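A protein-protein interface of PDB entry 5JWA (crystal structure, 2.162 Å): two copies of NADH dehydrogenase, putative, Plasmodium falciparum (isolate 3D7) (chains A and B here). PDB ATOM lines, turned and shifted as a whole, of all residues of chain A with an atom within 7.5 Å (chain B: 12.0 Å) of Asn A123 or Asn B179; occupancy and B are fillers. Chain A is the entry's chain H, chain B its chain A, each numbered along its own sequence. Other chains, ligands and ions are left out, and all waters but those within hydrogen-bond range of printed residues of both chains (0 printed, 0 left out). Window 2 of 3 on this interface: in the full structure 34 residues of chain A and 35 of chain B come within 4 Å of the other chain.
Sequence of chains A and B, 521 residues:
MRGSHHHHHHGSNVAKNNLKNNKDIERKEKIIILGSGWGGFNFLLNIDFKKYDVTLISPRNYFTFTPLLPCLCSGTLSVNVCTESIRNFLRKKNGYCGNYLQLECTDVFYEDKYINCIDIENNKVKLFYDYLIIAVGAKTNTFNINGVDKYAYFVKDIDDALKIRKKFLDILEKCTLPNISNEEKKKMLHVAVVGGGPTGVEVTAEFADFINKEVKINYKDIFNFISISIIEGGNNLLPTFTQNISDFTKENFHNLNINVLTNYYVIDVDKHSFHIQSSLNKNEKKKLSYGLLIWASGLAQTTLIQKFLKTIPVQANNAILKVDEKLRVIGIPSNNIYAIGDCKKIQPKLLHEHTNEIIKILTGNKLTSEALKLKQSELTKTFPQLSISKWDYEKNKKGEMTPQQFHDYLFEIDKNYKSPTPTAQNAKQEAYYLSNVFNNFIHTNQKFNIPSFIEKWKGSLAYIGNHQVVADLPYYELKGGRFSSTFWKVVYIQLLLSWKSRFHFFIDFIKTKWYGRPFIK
Asn A123 touches just one residue of chain B: Asn B179 (3.8 Å).
Printed residues of chain A within 4 Å of Asn B179: Asp A119 and Asn A123.
No residue of chain B comes within 4 Å of Ile A118.
Asn A122 touches none of the printed residues of chain B.
Of the printed residues of chain A, Lys B174 touches Glu A121 (2.9 Å).
Of the printed residues of chain A, Leu B177 touches Leu A103 (3.7 Å) and Asp A119 (3.7 Å).
Of the printed residues of chain B, Leu A103 touches Leu B177 (3.7 Å).
The nearest residue of chain B that does not touch Asn A123 is Lys B174 (5.8 Å).
Among the printed residues, pairs that only touch across the chains: Leu A103 with Leu B177, Asp A119 with Leu B177 and Asn A123 with Asn B179.
N of Glu A121 sits at hydrogen-bond distance from OD2 of Asp A119, at 2.9 Å.
N of Asn A122 is in hydrogen-bond range of OD2 of Asp A119.
The side-chain carboxylate (OD2) of Asp A119 is in hydrogen-bond range of the backbone NH (N) of Asn A123 (2.7 Å).
Hydrophobic or aromatic side chains of chain B that line the printed part of chain A: Leu B177.
Hydrophobic or aromatic side chains of chain A that line the printed part of chain B: Leu A103.
Among the printed residues, Asp or Glu carboxylates within 4 Å of a Lys or Arg side-chain nitrogen of the other chain: Glu A121 with Lys B174 (2.9 Å).
The side-chain amide nitrogen (ND2) of Asn B179 is in hydrogen-bond range of the side-chain carboxylate (OD1) of Asp A119.
NZ of Lys B174 lies within salt-bridge range of OE1 of Glu A121, 2.9 Å away.
No position is printed for both chains.
Of the 5 pairs that touch across the chains among the printed residues, none has its exchanged pair printed and touching as well.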
ATOM      1  N   LEU A 103     -14.832  -7.065  21.359  1.00  0.00           N
ATOM      2  CA  LEU A 103     -13.860  -6.449  22.243  1.00  0.00           C
ATOM      3  C   LEU A 103     -12.946  -5.526  21.454  1.00  0.00           C
ATOM      4  O   LEU A 103     -12.738  -5.720  20.254  1.00  0.00           O
ATOM      5  CB  LEU A 103     -13.023  -7.512  22.945  1.00  0.00           C
ATOM      6  CG  LEU A 103     -13.771  -8.550  23.779  1.00  0.00           C
ATOM      7  CD1 LEU A 103     -12.847  -9.689  24.202  1.00  0.00           C
ATOM      8  CD2 LEU A 103     -14.414  -7.862  24.984  1.00  0.00           C
ATOM      9  N   GLU A 104     -12.402  -4.535  22.146  1.00  0.00           N
ATOM     10  CA  GLU A 104     -11.333  -3.700  21.622  1.00  0.00           C
ATOM     11  C   GLU A 104     -10.005  -4.148  22.219  1.00  0.00           C
ATOM     12  O   GLU A 104      -9.838  -4.116  23.440  1.00  0.00           O
ATOM     13  CB  GLU A 104     -11.591  -2.231  21.955  1.00  0.00           C
ATOM     14  CG  GLU A 104     -10.405  -1.323  21.680  1.00  0.00           C
ATOM     15  CD  GLU A 104     -10.602   0.095  22.197  1.00  0.00           C
ATOM     16  OE1 GLU A 104     -11.763   0.546  22.312  1.00  0.00           O
ATOM     17  OE2 GLU A 104      -9.585   0.760  22.490  1.00  0.00           O
ATOM     18  N   CYS A 117      -7.717  -7.058  26.135  1.00  0.00           N
ATOM     19  CA  CYS A 117      -8.830  -6.370  25.497  1.00  0.00           C
ATOM     20  C   CYS A 117      -9.738  -5.753  26.557  1.00  0.00           C
ATOM     21  O   CYS A 117      -9.639  -6.097  27.729  1.00  0.00           O
ATOM     22  CB  CYS A 117      -9.629  -7.327  24.614  1.00  0.00           C
ATOM     23  SG  CYS A 117      -8.662  -8.273  23.397  1.00  0.00           S
ATOM     24  N   ILE A 118     -10.608  -4.835  26.140  1.00  0.00           N
ATOM     25  CA  ILE A 118     -11.668  -4.315  26.996  1.00  0.00           C
ATOM     26  C   ILE A 118     -13.000  -4.474  26.296  1.00  0.00           C
ATOM     27  O   ILE A 118     -13.053  -4.482  25.063  1.00  0.00           O
ATOM     28  CB  ILE A 118     -11.485  -2.819  27.346  1.00  0.00           C
ATOM     29  CG1 ILE A 118     -11.321  -1.979  26.073  1.00  0.00           C
ATOM     30  CG2 ILE A 118     -10.314  -2.630  28.282  1.00  0.00           C
ATOM     31  CD1 ILE A 118     -11.417  -0.484  26.300  1.00  0.00           C
ATOM     32  N   ASP A 119     -14.073  -4.604  27.074  1.00  0.00           N
ATOM     33  CA  ASP A 119     -15.407  -4.586  26.503  1.00  0.00           C
ATOM     34  C   ASP A 119     -15.925  -3.165  26.554  1.00  0.00           C
ATOM     35  O   ASP A 119     -15.242  -2.271  27.036  1.00  0.00           O
ATOM     36  CB  ASP A 119     -16.365  -5.554  27.223  1.00  0.00           C
ATOM     37  CG  ASP A 119     -16.467  -5.311  28.740  1.00  0.00           C
ATOM     38  OD1 ASP A 119     -16.789  -6.280  29.461  1.00  0.00           O
ATOM     39  OD2 ASP A 119     -16.248  -4.175  29.221  1.00  0.00           O
ATOM     40  N   ILE A 120     -17.137  -2.970  26.061  1.00  0.00           N
ATOM     41  CA  ILE A 120     -17.769  -1.657  26.012  1.00  0.00           C
ATOM     42  C   ILE A 120     -17.901  -1.003  27.402  1.00  0.00           C
ATOM     43  O   ILE A 120     -18.073   0.203  27.515  1.00  0.00           O
ATOM     44  CB  ILE A 120     -19.164  -1.771  25.345  1.00  0.00           C
ATOM     45  CG1 ILE A 120     -19.633  -0.412  24.806  1.00  0.00           C
ATOM     46  CG2 ILE A 120     -20.173  -2.438  26.292  1.00  0.00           C
ATOM     47  CD1 ILE A 120     -18.766   0.120  23.681  1.00  0.00           C
ATOM     48  N   GLU A 121     -17.802  -1.791  28.463  1.00  0.00           N
ATOM     49  CA  GLU A 121     -17.923  -1.233  29.802  1.00  0.00           C
ATOM     50  C   GLU A 121     -16.575  -1.216  30.506  1.00  0.00           C
ATOM     51  O   GLU A 121     -16.503  -1.115  31.733  1.00  0.00           O
ATOM     52  CB  GLU A 121     -18.964  -2.011  30.607  1.00  0.00           C
ATOM     53  CG  GLU A 121     -20.387  -1.784  30.104  1.00  0.00           C
ATOM     54  CD  GLU A 121     -21.405  -2.738  30.713  1.00  0.00           C
ATOM     55  OE1 GLU A 121     -21.287  -3.966  30.495  1.00  0.00           O
ATOM     56  OE2 GLU A 121     -22.331  -2.252  31.400  1.00  0.00           O
ATOM     57  N   ASN A 122     -15.514  -1.307  29.705  1.00  0.00           N
ATOM     58  CA  ASN A 122     -14.132  -1.209  30.173  1.00  0.00           C
ATOM     59  C   ASN A 122     -13.693  -2.325  31.100  1.00  0.00           C
ATOM     60  O   ASN A 122     -12.755  -2.156  31.861  1.00  0.00           O
ATOM     61  CB  ASN A 122     -13.895   0.135  30.871  1.00  0.00           C
ATOM     62  CG  ASN A 122     -13.389   1.197  29.923  1.00  0.00           C
ATOM     63  OD1 ASN A 122     -12.197   1.518  29.909  1.00  0.00           O
ATOM     64  ND2 ASN A 122     -14.285   1.733  29.109  1.00  0.00           N
ATOM     65  N   ASN A 123     -14.352  -3.471  31.033  1.00  0.00           N
ATOM     66  CA  ASN A 123     -13.850  -4.624  31.759  1.00  0.00           C
ATOM     67  C   ASN A 123     -12.706  -5.266  30.968  1.00  0.00           C
ATOM     68  O   ASN A 123     -12.872  -5.590  29.788  1.00  0.00           O
ATOM     69  CB  ASN A 123     -14.973  -5.633  32.012  1.00  0.00           C
ATOM     70  CG  ASN A 123     -16.152  -5.017  32.742  1.00  0.00           C
ATOM     71  OD1 ASN A 123     -15.990  -4.446  33.820  1.00  0.00           O
ATOM     72  ND2 ASN A 123     -17.339  -5.105  32.143  1.00  0.00           N
ATOM     73  N   LYS A 124     -11.552  -5.443  31.609  1.00  0.00           N
ATOM     74  CA  LYS A 124     -10.405  -6.063  30.953  1.00  0.00           C
ATOM     75  C   LYS A 124     -10.617  -7.558  30.748  1.00  0.00           C
ATOM     76  O   LYS A 124     -11.278  -8.218  31.547  1.00  0.00           O
ATOM     77  CB  LYS A 124      -9.130  -5.819  31.766  1.00  0.00           C
ATOM     78  CG  LYS A 124      -7.842  -6.297  31.094  1.00  0.00           C
ATOM     79  CD  LYS A 124      -6.637  -6.170  32.022  1.00  0.00           C
ATOM     80  CE  LYS A 124      -6.375  -4.719  32.409  1.00  0.00           C
ATOM     81  NZ  LYS A 124      -4.997  -4.509  32.952  1.00  0.00           N
ATOM     82  N   VAL A 125     -10.066  -8.087  29.661  1.00  0.00           N
ATOM     83  CA  VAL A 125     -10.104  -9.520  29.390  1.00  0.00           C
ATOM     84  C   VAL A 125      -8.816  -9.951  28.693  1.00  0.00           C
ATOM     85  O   VAL A 125      -8.314  -9.266  27.792  1.00  0.00           O
ATOM     86  CB  VAL A 125     -11.342  -9.903  28.541  1.00  0.00           C
ATOM     87  CG1 VAL A 125     -11.767  -8.743  27.682  1.00  0.00           C
ATOM     88  CG2 VAL A 125     -11.093 -11.162  27.710  1.00  0.00           C
ATOM     89  N   LYS A 126      -8.269 -11.079  29.135  1.00  0.00           N
ATOM     90  CA  LYS A 126      -6.969 -11.534  28.674  1.00  0.00           C
ATOM     91  C   LYS A 126      -7.130 -12.789  27.829  1.00  0.00           C
ATOM     92  O   LYS A 126      -7.874 -13.700  28.201  1.00  0.00           O
ATOM     93  CB  LYS A 126      -6.048 -11.793  29.865  1.00  0.00           C
ATOM     94  CG  LYS A 126      -4.731 -12.477  29.517  1.00  0.00           C
ATOM     95  CD  LYS A 126      -3.905 -12.777  30.769  1.00  0.00           C
ATOM     96  CE  LYS A 126      -2.564 -13.420  30.397  1.00  0.00           C
ATOM     97  NZ  LYS A 126      -1.791 -13.946  31.561  1.00  0.00           N
ATOM     98  N   ASP B 170     -27.101  -5.989  21.919  1.00  0.00           N
ATOM     99  CA  ASP B 170     -25.985  -5.686  22.811  1.00  0.00           C
ATOM    100  C   ASP B 170     -25.868  -6.708  23.944  1.00  0.00           C
ATOM    101  O   ASP B 170     -24.755  -7.053  24.348  1.00  0.00           O
ATOM    102  CB  ASP B 170     -26.115  -4.295  23.435  1.00  0.00           C
ATOM    103  CG  ASP B 170     -25.762  -3.178  22.484  1.00  0.00           C
ATOM    104  OD1 ASP B 170     -26.150  -2.027  22.797  1.00  0.00           O
ATOM    105  OD2 ASP B 170     -25.121  -3.424  21.433  1.00  0.00           O
ATOM    106  N   ILE B 171     -27.002  -7.164  24.479  1.00  0.00           N
ATOM    107  CA  ILE B 171     -26.970  -8.098  25.601  1.00  0.00           C
ATOM    108  C   ILE B 171     -26.438  -9.450  25.148  1.00  0.00           C
ATOM    109  O   ILE B 171     -25.661 -10.078  25.860  1.00  0.00           O
ATOM    110  CB  ILE B 171     -28.366  -8.284  26.256  1.00  0.00           C
ATOM    111  CG1 ILE B 171     -28.826  -6.997  26.933  1.00  0.00           C
ATOM    112  CG2 ILE B 171     -28.329  -9.395  27.300  1.00  0.00           C
ATOM    113  CD1 ILE B 171     -30.332  -6.949  27.171  1.00  0.00           C
ATOM    114  N   LEU B 172     -26.850  -9.894  23.964  1.00  0.00           N
ATOM    115  CA  LEU B 172     -26.339 -11.145  23.384  1.00  0.00           C
ATOM    116  C   LEU B 172     -24.804 -11.166  23.251  1.00  0.00           C
ATOM    117  O   LEU B 172     -24.149 -12.155  23.584  1.00  0.00           O
ATOM    118  CB  LEU B 172     -26.949 -11.378  22.003  1.00  0.00           C
ATOM    119  CG  LEU B 172     -28.462 -11.545  21.879  1.00  0.00           C
ATOM    120  CD1 LEU B 172     -28.830 -11.737  20.405  1.00  0.00           C
ATOM    121  CD2 LEU B 172     -28.941 -12.726  22.723  1.00  0.00           C
ATOM    122  N   GLU B 173     -24.245 -10.086  22.718  1.00  0.00           N
ATOM    123  CA  GLU B 173     -22.799  -9.990  22.556  1.00  0.00           C
ATOM    124  C   GLU B 173     -22.107  -9.964  23.918  1.00  0.00           C
ATOM    125  O   GLU B 173     -21.111 -10.650  24.119  1.00  0.00           O
ATOM    126  CB  GLU B 173     -22.419  -8.754  21.743  1.00  0.00           C
ATOM    127  CG  GLU B 173     -22.673  -8.905  20.239  1.00  0.00           C
ATOM    128  CD  GLU B 173     -22.023 -10.148  19.634  1.00  0.00           C
ATOM    129  OE1 GLU B 173     -22.557 -10.682  18.634  1.00  0.00           O
ATOM    130  OE2 GLU B 173     -20.983 -10.610  20.164  1.00  0.00           O
ATOM    131  N   LYS B 174     -22.647  -9.179  24.849  1.00  0.00           N
ATOM    132  CA  LYS B 174     -22.092  -9.097  26.189  1.00  0.00           C
ATOM    133  C   LYS B 174     -22.036 -10.473  26.857  1.00  0.00           C
ATOM    134  O   LYS B 174     -21.034 -10.837  27.494  1.00  0.00           O
ATOM    135  CB  LYS B 174     -22.911  -8.126  27.042  1.00  0.00           C
ATOM    136  CG  LYS B 174     -22.369  -7.954  28.450  1.00  0.00           C
ATOM    137  CD  LYS B 174     -23.056  -6.809  29.174  1.00  0.00           C
ATOM    138  CE  LYS B 174     -22.652  -6.761  30.643  1.00  0.00           C
ATOM    139  NZ  LYS B 174     -23.409  -5.707  31.387  1.00  0.00           N
ATOM    140  N   CYS B 175     -23.103 -11.249  26.699  1.00  0.00           N
ATOM    141  CA  CYS B 175     -23.184 -12.574  27.318  1.00  0.00           C
ATOM    142  C   CYS B 175     -22.401 -13.655  26.582  1.00  0.00           C
ATOM    143  O   CYS B 175     -22.388 -14.814  27.000  1.00  0.00           O
ATOM    144  CB  CYS B 175     -24.646 -13.004  27.432  1.00  0.00           C
ATOM    145  SG  CYS B 175     -25.559 -12.011  28.620  1.00  0.00           S
ATOM    146  N   THR B 176     -21.766 -13.289  25.475  1.00  0.00           N
ATOM    147  CA  THR B 176     -20.903 -14.208  24.754  1.00  0.00           C
ATOM    148  C   THR B 176     -19.452 -14.048  25.272  1.00  0.00           C
ATOM    149  O   THR B 176     -18.606 -14.887  25.021  1.00  0.00           O
ATOM    150  CB  THR B 176     -21.001 -13.963  23.216  1.00  0.00           C
ATOM    151  OG1 THR B 176     -22.338 -14.241  22.781  1.00  0.00           O
ATOM    152  CG2 THR B 176     -20.059 -14.870  22.421  1.00  0.00           C
ATOM    153  N   LEU B 177     -19.187 -12.982  26.022  1.00  0.00           N
ATOM    154  CA  LEU B 177     -17.852 -12.738  26.569  1.00  0.00           C
ATOM    155  C   LEU B 177     -17.495 -13.735  27.674  1.00  0.00           C
ATOM    156  O   LEU B 177     -18.371 -14.193  28.400  1.00  0.00           O
ATOM    157  CB  LEU B 177     -17.754 -11.316  27.104  1.00  0.00           C
ATOM    158  CG  LEU B 177     -18.054 -10.248  26.064  1.00  0.00           C
ATOM    159  CD1 LEU B 177     -17.973  -8.850  26.680  1.00  0.00           C
ATOM    160  CD2 LEU B 177     -17.084 -10.408  24.905  1.00  0.00           C
ATOM    161  N   PRO B 178     -16.196 -14.066  27.810  1.00  0.00           N
ATOM    162  CA  PRO B 178     -15.782 -15.088  28.787  1.00  0.00           C
ATOM    163  C   PRO B 178     -15.801 -14.573  30.229  1.00  0.00           C
ATOM    164  O   PRO B 178     -15.714 -15.364  31.166  1.00  0.00           O
ATOM    165  CB  PRO B 178     -14.352 -15.433  28.341  1.00  0.00           C
ATOM    166  CG  PRO B 178     -13.841 -14.156  27.744  1.00  0.00           C
ATOM    167  CD  PRO B 178     -15.045 -13.472  27.101  1.00  0.00           C
ATOM    168  N   ASN B 179     -15.943 -13.265  30.411  1.00  0.00           N
ATOM    169  CA  ASN B 179     -15.921 -12.698  31.751  1.00  0.00           C
ATOM    170  C   ASN B 179     -17.303 -12.647  32.446  1.00  0.00           C
ATOM    171  O   ASN B 179     -17.547 -11.760  33.265  1.00  0.00           O
ATOM    172  CB  ASN B 179     -15.298 -11.289  31.709  1.00  0.00           C
ATOM    173  CG  ASN B 179     -16.038 -10.316  30.763  1.00  0.00           C
ATOM    174  OD1 ASN B 179     -17.085 -10.636  30.193  1.00  0.00           O
ATOM    175  ND2 ASN B 179     -15.489  -9.112  30.617  1.00  0.00           N
ATOM    176  N   ILE B 180     -18.193 -13.594  32.126  1.00  0.00           N
ATOM    177  CA  ILE B 180     -19.559 -13.600  32.668  1.00  0.00           C
ATOM    178  C   ILE B 180     -20.015 -14.981  33.145  1.00  0.00           C
ATOM    179  O   ILE B 180     -19.963 -15.947  32.394  1.00  0.00           O
ATOM    180  CB  ILE B 180     -20.597 -13.114  31.624  1.00  0.00           C
ATOM    181  CG1 ILE B 180     -20.066 -11.939  30.800  1.00  0.00           C
ATOM    182  CG2 ILE B 180     -21.908 -12.740  32.309  1.00  0.00           C
ATOM    183  CD1 ILE B 180     -20.078 -10.613  31.525  1.00  0.00           C
ATOM    184  N   SER B 181     -20.498 -15.069  34.381  1.00  0.00           N
ATOM    185  CA  SER B 181     -21.003 -16.341  34.916  1.00  0.00           C
ATOM    186  C   SER B 181     -22.338 -16.736  34.289  1.00  0.00           C
ATOM    187  O   SER B 181     -23.050 -15.894  33.755  1.00  0.00           O
ATOM    188  CB  SER B 181     -21.166 -16.264  36.436  1.00  0.00           C
ATOM    189  OG  SER B 181     -22.178 -15.335  36.793  1.00  0.00           O
ATOM    190  N   ASN B 182     -22.674 -18.019  34.374  1.00  0.00           N
ATOM    191  CA  ASN B 182     -23.932 -18.510  33.837  1.00  0.00           C
ATOM    192  C   ASN B 182     -25.145 -17.900  34.543  1.00  0.00           C
ATOM    193  O   ASN B 182     -26.193 -17.674  33.923  1.00  0.00           O
ATOM    194  CB  ASN B 182     -23.964 -20.032  33.915  1.00  0.00           C
ATOM    195  CG  ASN B 182     -23.123 -20.674  32.835  1.00  0.00           C
ATOM    196  OD1 ASN B 182     -22.428 -19.984  32.088  1.00  0.00           O
ATOM    197  ND2 ASN B 182     -23.186 -21.992  32.732  1.00  0.00           N
ATOM    198  N   GLU B 183     -24.982 -17.612  35.833  1.00  0.00           N
ATOM    199  CA  GLU B 183     -26.028 -16.987  36.630  1.00  0.00           C
ATOM    200  C   GLU B 183     -26.272 -15.554  36.172  1.00  0.00           C
ATOM    201  O   GLU B 183     -27.413 -15.113  36.073  1.00  0.00           O
ATOM    202  CB  GLU B 183     -25.657 -17.011  38.118  1.00  0.00           C
ATOM    203  CG  GLU B 183     -26.650 -16.302  39.030  1.00  0.00           C
ATOM    204  CD  GLU B 183     -26.134 -16.146  40.458  1.00  0.00           C
ATOM    205  OE1 GLU B 183     -24.930 -16.416  40.692  1.00  0.00           O
ATOM    206  OE2 GLU B 183     -26.933 -15.754  41.344  1.00  0.00           O
ATOM    207  N   GLU B 184     -25.200 -14.824  35.898  1.00  0.00           N
ATOM    208  CA  GLU B 184     -25.343 -13.461  35.413  1.00  0.00           C
ATOM    209  C   GLU B 184     -26.029 -13.465  34.054  1.00  0.00           C
ATOM    210  O   GLU B 184     -26.829 -12.581  33.757  1.00  0.00           O
ATOM    211  CB  GLU B 184     -23.993 -12.766  35.298  1.00  0.00           C
ATOM    212  CG  GLU B 184     -23.352 -12.354  36.596  1.00  0.00           C
ATOM    213  CD  GLU B 184     -21.909 -11.914  36.373  1.00  0.00           C
ATOM    214  OE1 GLU B 184     -21.662 -10.688  36.286  1.00  0.00           O
ATOM    215  OE2 GLU B 184     -21.029 -12.802  36.250  1.00  0.00           O
ATOM    216  N   LYS B 185     -25.709 -14.475  33.249  1.00  0.00           N
ATOM    217  CA  LYS B 185     -26.272 -14.614  31.912  1.00  0.00           C
ATOM    218  C   LYS B 185     -27.781 -14.804  31.948  1.00  0.00           C
ATOM    219  O   LYS B 185     -28.516 -14.103  31.241  1.00  0.00           O
ATOM    220  CB  LYS B 185     -25.618 -15.782  31.171  1.00  0.00           C
ATOM    221  CG  LYS B 185     -24.196 -15.500  30.725  1.00  0.00           C
ATOM    222  CD  LYS B 185     -23.636 -16.638  29.881  1.00  0.00           C
ATOM    223  CE  LYS B 185     -22.138 -16.467  29.675  1.00  0.00           C
ATOM    224  NZ  LYS B 185     -21.574 -17.573  28.847  1.00  0.00           N
ATOM    225  N   LYS B 186     -28.240 -15.759  32.758  1.00  0.00           N
ATOM    226  CA  LYS B 186     -29.669 -15.988  32.931  1.00  0.00           C
ATOM    227  C   LYS B 186     -30.402 -14.707  33.374  1.00  0.00           C
ATOM    228  O   LYS B 186     -31.545 -14.464  32.978  1.00  0.00           O
ATOM    229  CB  LYS B 186     -29.913 -17.103  33.948  1.00  0.00           C
ATOM    230  CG  LYS B 186     -29.394 -18.470  33.528  1.00  0.00           C
ATOM    231  CD  LYS B 186     -29.682 -19.501  34.623  1.00  0.00           C
ATOM    232  CE  LYS B 186     -28.836 -20.751  34.464  1.00  0.00           C
ATOM    233  NZ  LYS B 186     -28.854 -21.585  35.703  1.00  0.00           N
ATOM    234  N   MET B 188     -29.327 -11.511  32.751  1.00  0.00           N
ATOM    235  CA  MET B 188     -29.237 -10.485  31.716  1.00  0.00           C
ATOM    236  C   MET B 188     -30.041 -10.835  30.467  1.00  0.00           C
ATOM    237  O   MET B 188     -30.449  -9.957  29.722  1.00  0.00           O
ATOM    238  CB  MET B 188     -27.773 -10.245  31.330  1.00  0.00           C
ATOM    239  CG  MET B 188     -27.086  -9.189  32.167  1.00  0.00           C
ATOM    240  SD  MET B 188     -25.329  -9.002  31.761  1.00  0.00           S
ATOM    241  CE  MET B 188     -24.695 -10.579  32.327  1.00  0.00           C
ATOM    242  N   LEU B 189     -30.254 -12.117  30.235  1.00  0.00           N
ATOM    243  CA  LEU B 189     -30.951 -12.551  29.047  1.00  0.00           C
ATOM    244  C   LEU B 189     -32.429 -12.800  29.317  1.00  0.00           C
ATOM    245  O   LEU B 189     -33.081 -13.535  28.585  1.00  0.00           O
ATOM    246  CB  LEU B 189     -30.282 -13.810  28.486  1.00  0.00           C
ATOM    247  CG  LEU B 189     -28.836 -13.621  28.020  1.00  0.00           C
ATOM    248  CD1 LEU B 189     -28.137 -14.963  27.905  1.00  0.00           C
ATOM    249  CD2 LEU B 189     -28.817 -12.897  26.674  1.00  0.00           C
ATOM    250  N   ILE B 222     -25.591 -19.734  24.266  1.00  0.00           N
ATOM    251  CA  ILE B 222     -26.371 -19.017  25.282  1.00  0.00           C
ATOM    252  C   ILE B 222     -27.874 -19.092  25.030  1.00  0.00           C
ATOM    253  O   ILE B 222     -28.646 -18.482  25.763  1.00  0.00           O
ATOM    254  CB  ILE B 222     -25.978 -17.529  25.397  1.00  0.00           C
ATOM    255  CG1 ILE B 222     -26.170 -16.807  24.065  1.00  0.00           C
ATOM    256  CG2 ILE B 222     -24.539 -17.362  25.882  1.00  0.00           C
ATOM    257  CD1 ILE B 222     -25.890 -15.311  24.170  1.00  0.00           C
ATOM    258  N   PHE B 225     -30.060 -19.894  27.983  1.00  0.00           N
ATOM    259  CA  PHE B 225     -30.108 -18.952  29.103  1.00  0.00           C
ATOM    260  C   PHE B 225     -31.132 -17.840  28.898  1.00  0.00           C
ATOM    261  O   PHE B 225     -31.420 -17.079  29.825  1.00  0.00           O
ATOM    262  CB  PHE B 225     -28.734 -18.322  29.342  1.00  0.00           C
ATOM    263  CG  PHE B 225     -27.659 -19.314  29.663  1.00  0.00           C
ATOM    264  CD1 PHE B 225     -27.934 -20.436  30.434  1.00  0.00           C
ATOM    265  CD2 PHE B 225     -26.366 -19.126  29.194  1.00  0.00           C
ATOM    266  CE1 PHE B 225     -26.940 -21.354  30.732  1.00  0.00           C
ATOM    267  CE2 PHE B 225     -25.360 -20.043  29.493  1.00  0.00           C
ATOM    268  CZ  PHE B 225     -25.650 -21.154  30.260  1.00  0.00           C
ATOM    269  N   LYS B 271     -32.598  -0.977  38.648  1.00  0.00           N
ATOM    270  CA  LYS B 271     -31.675  -1.130  37.527  1.00  0.00           C
ATOM    271  C   LYS B 271     -31.563  -2.564  37.004  1.00  0.00           C
ATOM    272  O   LYS B 271     -31.499  -2.773  35.794  1.00  0.00           O
ATOM    273  CB  LYS B 271     -30.289  -0.615  37.912  1.00  0.00           C
ATOM    274  CG  LYS B 271     -29.325  -0.475  36.742  1.00  0.00           C
ATOM    275  CD  LYS B 271     -28.250   0.562  37.068  1.00  0.00           C
ATOM    276  CE  LYS B 271     -27.081   0.496  36.097  1.00  0.00           C
ATOM    277  NZ  LYS B 271     -26.300  -0.753  36.304  1.00  0.00           N
ATOM    278  N   HIS B 272     -31.552  -3.547  37.897  1.00  0.00           N
ATOM    279  CA  HIS B 272     -31.358  -4.937  37.480  1.00  0.00           C
ATOM    280  C   HIS B 272     -32.476  -5.893  37.893  1.00  0.00           C
ATOM    281  O   HIS B 272     -32.401  -7.093  37.623  1.00  0.00           O
ATOM    282  CB  HIS B 272     -30.027  -5.470  38.021  1.00  0.00           C
ATOM    283  CG  HIS B 272     -28.835  -4.747  37.482  1.00  0.00           C
ATOM    284  ND1 HIS B 272     -28.415  -4.877  36.176  1.00  0.00           N
ATOM    285  CD2 HIS B 272     -27.987  -3.868  38.067  1.00  0.00           C
ATOM    286  CE1 HIS B 272     -27.353  -4.117  35.980  1.00  0.00           C
ATOM    287  NE2 HIS B 272     -27.071  -3.496  37.112  1.00  0.00           N
